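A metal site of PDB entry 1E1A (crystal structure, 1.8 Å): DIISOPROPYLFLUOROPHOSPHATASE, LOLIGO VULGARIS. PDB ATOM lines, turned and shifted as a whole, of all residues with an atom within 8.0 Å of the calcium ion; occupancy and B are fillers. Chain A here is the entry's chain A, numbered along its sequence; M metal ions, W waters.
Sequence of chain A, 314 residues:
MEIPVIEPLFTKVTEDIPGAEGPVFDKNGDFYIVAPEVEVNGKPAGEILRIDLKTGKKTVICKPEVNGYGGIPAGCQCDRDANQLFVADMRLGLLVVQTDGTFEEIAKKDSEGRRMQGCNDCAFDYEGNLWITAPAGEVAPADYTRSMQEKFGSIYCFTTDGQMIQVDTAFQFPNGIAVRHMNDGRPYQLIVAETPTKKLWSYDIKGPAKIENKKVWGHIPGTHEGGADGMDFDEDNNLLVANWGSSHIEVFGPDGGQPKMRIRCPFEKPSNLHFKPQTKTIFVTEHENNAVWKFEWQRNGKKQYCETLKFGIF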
ATOM      1  N   GLU A  21     -20.176 -13.924 -18.618  1.00  0.00           N
ATOM      2  CA  GLU A  21     -19.652 -14.303 -17.305  1.00  0.00           C
ATOM      3  C   GLU A  21     -19.841 -13.233 -16.238  1.00  0.00           C
ATOM      4  O   GLU A  21     -20.429 -12.181 -16.475  1.00  0.00           O
ATOM      5  CB  GLU A  21     -18.148 -14.580 -17.455  1.00  0.00           C
ATOM      6  CG  GLU A  21     -17.757 -16.047 -17.546  1.00  0.00           C
ATOM      7  CD  GLU A  21     -17.527 -16.679 -16.183  1.00  0.00           C
ATOM      8  OE1 GLU A  21     -18.089 -16.205 -15.178  1.00  0.00           O
ATOM      9  OE2 GLU A  21     -16.757 -17.672 -16.119  1.00  0.00           O
ATOM     10  N   GLY A  22     -19.307 -13.552 -15.054  1.00  0.00           N
ATOM     11  CA  GLY A  22     -19.326 -12.659 -13.902  1.00  0.00           C
ATOM     12  C   GLY A  22     -20.555 -11.835 -13.586  1.00  0.00           C
ATOM     13  O   GLY A  22     -20.430 -10.629 -13.411  1.00  0.00           O
ATOM     14  N   PRO A  23     -21.747 -12.448 -13.511  1.00  0.00           N
ATOM     15  CA  PRO A  23     -22.959 -11.675 -13.188  1.00  0.00           C
ATOM     16  C   PRO A  23     -22.801 -11.088 -11.784  1.00  0.00           C
ATOM     17  O   PRO A  23     -22.338 -11.759 -10.854  1.00  0.00           O
ATOM     18  CB  PRO A  23     -24.069 -12.731 -13.248  1.00  0.00           C
ATOM     19  CG  PRO A  23     -23.363 -13.991 -12.873  1.00  0.00           C
ATOM     20  CD  PRO A  23     -22.076 -13.884 -13.639  1.00  0.00           C
ATOM     21  N   VAL A  24     -23.161  -9.821 -11.624  1.00  0.00           N
ATOM     22  CA  VAL A  24     -23.017  -9.172 -10.335  1.00  0.00           C
ATOM     23  C   VAL A  24     -23.921  -7.967 -10.210  1.00  0.00           C
ATOM     24  O   VAL A  24     -24.314  -7.364 -11.211  1.00  0.00           O
ATOM     25  CB  VAL A  24     -21.523  -8.731 -10.106  1.00  0.00           C
ATOM     26  CG1 VAL A  24     -21.119  -7.631 -11.092  1.00  0.00           C
ATOM     27  CG2 VAL A  24     -21.297  -8.284  -8.671  1.00  0.00           C
ATOM     28  N   PHE A  25     -24.336  -7.673  -8.987  1.00  0.00           N
ATOM     29  CA  PHE A  25     -25.168  -6.514  -8.687  1.00  0.00           C
ATOM     30  C   PHE A  25     -24.331  -5.575  -7.823  1.00  0.00           C
ATOM     31  O   PHE A  25     -23.617  -6.032  -6.928  1.00  0.00           O
ATOM     32  CB  PHE A  25     -26.411  -6.932  -7.887  1.00  0.00           C
ATOM     33  CG  PHE A  25     -27.520  -7.499  -8.733  1.00  0.00           C
ATOM     34  CD1 PHE A  25     -28.471  -6.656  -9.290  1.00  0.00           C
ATOM     35  CD2 PHE A  25     -27.621  -8.869  -8.938  1.00  0.00           C
ATOM     36  CE1 PHE A  25     -29.516  -7.171 -10.055  1.00  0.00           C
ATOM     37  CE2 PHE A  25     -28.664  -9.394  -9.699  1.00  0.00           C
ATOM     38  CZ  PHE A  25     -29.617  -8.542 -10.260  1.00  0.00           C
ATOM     39  N   CYS A  76     -16.577 -11.197 -11.320  1.00  0.00           N
ATOM     40  CA  CYS A  76     -16.765  -9.946 -10.580  1.00  0.00           C
ATOM     41  C   CYS A  76     -17.255 -10.079  -9.138  1.00  0.00           C
ATOM     42  O   CYS A  76     -17.929 -11.052  -8.781  1.00  0.00           O
ATOM     43  CB  CYS A  76     -17.792  -9.052 -11.304  1.00  0.00           C
ATOM     44  SG  CYS A  76     -17.550  -8.820 -13.078  1.00  0.00           S
ATOM     45  N   GLN A  77     -16.942  -9.062  -8.344  1.00  0.00           N
ATOM     46  CA  GLN A  77     -17.360  -8.957  -6.953  1.00  0.00           C
ATOM     47  C   GLN A  77     -17.522  -7.480  -6.704  1.00  0.00           C
ATOM     48  O   GLN A  77     -16.657  -6.690  -7.081  1.00  0.00           O
ATOM     49  CB  GLN A  77     -16.308  -9.516  -5.983  1.00  0.00           C
ATOM     50  CG  GLN A  77     -16.294 -11.019  -5.830  1.00  0.00           C
ATOM     51  CD  GLN A  77     -17.581 -11.587  -5.254  1.00  0.00           C
ATOM     52  OE1 GLN A  77     -18.492 -11.981  -5.994  1.00  0.00           O
ATOM     53  NE2 GLN A  77     -17.660 -11.657  -3.939  1.00  0.00           N
ATOM     54  N   ASP A 121     -12.193 -15.785 -11.506  1.00  0.00           N
ATOM     55  CA  ASP A 121     -13.289 -15.450 -10.613  1.00  0.00           C
ATOM     56  C   ASP A 121     -12.731 -15.047  -9.248  1.00  0.00           C
ATOM     57  O   ASP A 121     -11.549 -15.274  -8.967  1.00  0.00           O
ATOM     58  CB  ASP A 121     -14.288 -16.604 -10.483  1.00  0.00           C
ATOM     59  CG  ASP A 121     -15.731 -16.125 -10.255  1.00  0.00           C
ATOM     60  OD1 ASP A 121     -15.949 -14.924  -9.967  1.00  0.00           O
ATOM     61  OD2 ASP A 121     -16.658 -16.949 -10.370  1.00  0.00           O
ATOM     62  N   CYS A 122     -13.571 -14.435  -8.428  1.00  0.00           N
ATOM     63  CA  CYS A 122     -13.157 -14.001  -7.106  1.00  0.00           C
ATOM     64  C   CYS A 122     -14.333 -13.973  -6.155  1.00  0.00           C
ATOM     65  O   CYS A 122     -15.501 -14.008  -6.574  1.00  0.00           O
ATOM     66  CB  CYS A 122     -12.478 -12.622  -7.186  1.00  0.00           C
ATOM     67  SG  CYS A 122     -13.463 -11.300  -7.945  1.00  0.00           S
ATOM     68  N   ILE A 177     -15.209 -19.744  -7.135  1.00  0.00           N
ATOM     69  CA  ILE A 177     -14.680 -19.662  -5.781  1.00  0.00           C
ATOM     70  C   ILE A 177     -15.739 -19.064  -4.859  1.00  0.00           C
ATOM     71  O   ILE A 177     -16.522 -18.215  -5.277  1.00  0.00           O
ATOM     72  CB  ILE A 177     -13.351 -18.844  -5.787  1.00  0.00           C
ATOM     73  CG1 ILE A 177     -12.659 -18.887  -4.421  1.00  0.00           C
ATOM     74  CG2 ILE A 177     -13.604 -17.418  -6.254  1.00  0.00           C
ATOM     75  CD1 ILE A 177     -11.187 -18.515  -4.470  1.00  0.00           C
ATOM     76  N   GLY A 230     -18.865 -21.382 -12.205  1.00  0.00           N
ATOM     77  CA  GLY A 230     -19.173 -20.423 -11.151  1.00  0.00           C
ATOM     78  C   GLY A 230     -19.986 -20.993 -10.012  1.00  0.00           C
ATOM     79  O   GLY A 230     -20.690 -21.986 -10.178  1.00  0.00           O
ATOM     80  N   MET A 231     -19.921 -20.331  -8.850  1.00  0.00           N
ATOM     81  CA  MET A 231     -20.646 -20.781  -7.667  1.00  0.00           C
ATOM     82  C   MET A 231     -21.047 -19.632  -6.735  1.00  0.00           C
ATOM     83  O   MET A 231     -20.472 -18.542  -6.775  1.00  0.00           O
ATOM     84  CB  MET A 231     -19.798 -21.780  -6.876  1.00  0.00           C
ATOM     85  CG  MET A 231     -18.494 -21.193  -6.319  1.00  0.00           C
ATOM     86  SD  MET A 231     -17.479 -22.338  -5.366  1.00  0.00           S
ATOM     87  CE  MET A 231     -17.215 -23.630  -6.570  1.00  0.00           C
ATOM     88  N   ASP A 232     -22.023 -19.921  -5.877  1.00  0.00           N
ATOM     89  CA  ASP A 232     -22.518 -18.989  -4.866  1.00  0.00           C
ATOM     90  C   ASP A 232     -23.349 -19.747  -3.842  1.00  0.00           C
ATOM     91  O   ASP A 232     -23.960 -20.775  -4.156  1.00  0.00           O
ATOM     92  CB  ASP A 232     -23.370 -17.865  -5.473  1.00  0.00           C
ATOM     93  CG  ASP A 232     -22.571 -16.599  -5.749  1.00  0.00           C
ATOM     94  OD1 ASP A 232     -21.623 -16.281  -4.994  1.00  0.00           O
ATOM     95  OD2 ASP A 232     -22.887 -15.891  -6.725  1.00  0.00           O
ATOM     96  N   PHE A 233     -23.346 -19.247  -2.603  1.00  0.00           N
ATOM     97  CA  PHE A 233     -24.110 -19.868  -1.515  1.00  0.00           C
ATOM     98  C   PHE A 233     -25.491 -19.246  -1.379  1.00  0.00           C
ATOM     99  O   PHE A 233     -25.666 -18.056  -1.673  1.00  0.00           O
ATOM    100  CB  PHE A 233     -23.408 -19.637  -0.170  1.00  0.00           C
ATOM    101  CG  PHE A 233     -22.256 -20.559   0.089  1.00  0.00           C
ATOM    102  CD1 PHE A 233     -22.465 -21.915   0.337  1.00  0.00           C
ATOM    103  CD2 PHE A 233     -20.953 -20.071   0.136  1.00  0.00           C
ATOM    104  CE1 PHE A 233     -21.409 -22.765   0.622  1.00  0.00           C
ATOM    105  CE2 PHE A 233     -19.885 -20.926   0.427  1.00  0.00           C
ATOM    106  CZ  PHE A 233     -20.109 -22.274   0.677  1.00  0.00           C
ATOM    107  N   LEU A 240     -24.555 -23.563  -4.754  1.00  0.00           N
ATOM    108  CA  LEU A 240     -25.038 -23.791  -6.116  1.00  0.00           C
ATOM    109  C   LEU A 240     -23.841 -23.625  -7.046  1.00  0.00           C
ATOM    110  O   LEU A 240     -23.119 -22.634  -6.977  1.00  0.00           O
ATOM    111  CB  LEU A 240     -26.184 -22.835  -6.482  1.00  0.00           C
ATOM    112  CG  LEU A 240     -27.483 -23.112  -5.721  1.00  0.00           C
ATOM    113  CD1 LEU A 240     -27.410 -22.528  -4.323  1.00  0.00           C
ATOM    114  CD2 LEU A 240     -28.666 -22.539  -6.477  1.00  0.00           C
ATOM    115  N   ASN A 272     -21.874 -19.056 -14.995  1.00  0.00           N
ATOM    116  CA  ASN A 272     -21.796 -18.402 -13.708  1.00  0.00           C
ATOM    117  C   ASN A 272     -23.175 -17.962 -13.266  1.00  0.00           C
ATOM    118  O   ASN A 272     -24.112 -17.906 -14.075  1.00  0.00           O
ATOM    119  CB  ASN A 272     -20.835 -17.206 -13.767  1.00  0.00           C
ATOM    120  CG  ASN A 272     -19.961 -17.070 -12.525  1.00  0.00           C
ATOM    121  OD1 ASN A 272     -18.804 -16.655 -12.599  1.00  0.00           O
ATOM    122  ND2 ASN A 272     -20.526 -17.391 -11.357  1.00  0.00           N
ATOM    123  N   LEU A 273     -23.313 -17.654 -11.986  1.00  0.00           N
ATOM    124  CA  LEU A 273     -24.601 -17.243 -11.451  1.00  0.00           C
ATOM    125  C   LEU A 273     -24.445 -16.225 -10.330  1.00  0.00           C
ATOM    126  O   LEU A 273     -23.361 -16.058  -9.782  1.00  0.00           O
ATOM    127  CB  LEU A 273     -25.361 -18.485 -10.964  1.00  0.00           C
ATOM    128  CG  LEU A 273     -24.627 -19.447 -10.034  1.00  0.00           C
ATOM    129  CD1 LEU A 273     -24.779 -19.000  -8.604  1.00  0.00           C
ATOM    130  CD2 LEU A 273     -25.204 -20.846 -10.185  1.00  0.00           C
ATOM    131  N   HIS A 274     -25.542 -15.554 -10.012  1.00  0.00           N
ATOM    132  CA  HIS A 274     -25.554 -14.548  -8.957  1.00  0.00           C
ATOM    133  C   HIS A 274     -26.984 -14.247  -8.549  1.00  0.00           C
ATOM    134  O   HIS A 274     -27.884 -14.160  -9.383  1.00  0.00           O
ATOM    135  CB  HIS A 274     -24.895 -13.254  -9.469  1.00  0.00           C
ATOM    136  CG  HIS A 274     -24.229 -12.453  -8.392  1.00  0.00           C
ATOM    137  ND1 HIS A 274     -22.976 -12.774  -7.892  1.00  0.00           N
ATOM    138  CD2 HIS A 274     -24.612 -11.330  -7.743  1.00  0.00           C
ATOM    139  CE1 HIS A 274     -22.617 -11.873  -6.992  1.00  0.00           C
ATOM    140  NE2 HIS A 274     -23.594 -10.991  -6.881  1.00  0.00           N
ATOM    141  N   PHE A 275     -27.193 -14.140  -7.235  1.00  0.00           N
ATOM    142  CA  PHE A 275     -28.503 -13.822  -6.687  1.00  0.00           C
ATOM    143  C   PHE A 275     -28.726 -12.309  -6.721  1.00  0.00           C
ATOM    144  O   PHE A 275     -27.780 -11.536  -6.540  1.00  0.00           O
ATOM    145  CB  PHE A 275     -28.594 -14.227  -5.208  1.00  0.00           C
ATOM    146  CG  PHE A 275     -28.795 -15.686  -4.978  1.00  0.00           C
ATOM    147  CD1 PHE A 275     -27.702 -16.541  -4.887  1.00  0.00           C
ATOM    148  CD2 PHE A 275     -30.075 -16.207  -4.781  1.00  0.00           C
ATOM    149  CE1 PHE A 275     -27.877 -17.898  -4.592  1.00  0.00           C
ATOM    150  CE2 PHE A 275     -30.259 -17.566  -4.488  1.00  0.00           C
ATOM    151  CZ  PHE A 275     -29.159 -18.409  -4.400  1.00  0.00           C
ATOM    152  N   ILE A 282     -32.024 -15.984  -9.238  1.00  0.00           N
ATOM    153  CA  ILE A 282     -30.637 -16.275  -9.608  1.00  0.00           C
ATOM    154  C   ILE A 282     -30.463 -16.002 -11.089  1.00  0.00           C
ATOM    155  O   ILE A 282     -31.187 -16.532 -11.931  1.00  0.00           O
ATOM    156  CB  ILE A 282     -30.246 -17.741  -9.340  1.00  0.00           C
ATOM    157  CG1 ILE A 282     -30.324 -18.070  -7.857  1.00  0.00           C
ATOM    158  CG2 ILE A 282     -28.817 -17.999  -9.839  1.00  0.00           C
ATOM    159  CD1 ILE A 282     -29.942 -19.508  -7.536  1.00  0.00           C
ATOM    160  N   PHE A 283     -29.515 -15.117 -11.400  1.00  0.00           N
ATOM    161  CA  PHE A 283     -29.178 -14.784 -12.771  1.00  0.00           C
ATOM    162  C   PHE A 283     -28.084 -15.743 -13.199  1.00  0.00           C
ATOM    163  O   PHE A 283     -27.109 -15.950 -12.467  1.00  0.00           O
ATOM    164  CB  PHE A 283     -28.719 -13.325 -12.874  1.00  0.00           C
ATOM    165  CG  PHE A 283     -29.856 -12.354 -12.780  1.00  0.00           C
ATOM    166  CD1 PHE A 283     -30.463 -12.096 -11.550  1.00  0.00           C
ATOM    167  CD2 PHE A 283     -30.358 -11.740 -13.917  1.00  0.00           C
ATOM    168  CE1 PHE A 283     -31.574 -11.245 -11.472  1.00  0.00           C
ATOM    169  CE2 PHE A 283     -31.462 -10.897 -13.856  1.00  0.00           C
ATOM    170  CZ  PHE A 283     -32.077 -10.651 -12.623  1.00  0.00           C
ATOM    171  N   GLN A 304     -23.880 -10.990  -0.073  1.00  0.00           N
ATOM    172  CA  GLN A 304     -22.535 -10.751  -0.591  1.00  0.00           C
ATOM    173  C   GLN A 304     -21.900  -9.693   0.309  1.00  0.00           C
ATOM    174  O   GLN A 304     -22.578  -9.029   1.081  1.00  0.00           O
ATOM    175  CB  GLN A 304     -22.616 -10.245  -2.039  1.00  0.00           C
ATOM    176  CG  GLN A 304     -22.971 -11.331  -3.059  1.00  0.00           C
ATOM    177  CD  GLN A 304     -21.767 -12.167  -3.448  1.00  0.00           C
ATOM    178  OE1 GLN A 304     -21.618 -13.318  -3.030  1.00  0.00           O
ATOM    179  NE2 GLN A 304     -20.885 -11.586  -4.266  1.00  0.00           N
HETATM  180 CA    CA M   1     -21.788 -14.980  -8.421  1.00  0.00          CA
HETATM  181  O   HOH W   1     -20.328 -16.779  -8.779  1.00  0.00           O
HETATM  182  O   HOH W   2     -20.261 -14.476  -6.634  1.00  0.00           O
HETATM  183  O   HOH W   3     -20.905 -13.944 -10.253  1.00  0.00           O
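N of Leu 240 is in hydrogen-bond range of O of Asp 232 (2.9 Å). The backbone carbonyl oxygen of Pro 23 sits close to a ring nitrogen (ND1) of His 274, 3.2 Å away. The backbone carbonyl oxygen of His 274 sits at hydrogen-bond distance from the backbone NH of Phe 283, at 2.8 Å.
The calcium ion is bound by OD2 of Asp 232 (2.2 Å), water W3 (2.3 Å), O of Leu 273 (2.3 Å), water W1 (2.3 Å), water W2 (2.4 Å) and ND1 of His 274 (2.6 Å). The calcium ion has six donor atoms within binding distance.
Water W2 bridges the side-chain carboxylate (OD1) of Asp 232 (2.8 Å) and the side-chain amide oxygen (OE1) of Gln 77 (3.1 Å). Water W1 lies within hydrogen-bond range of ND2 of Asn 272 and O of Met 231.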
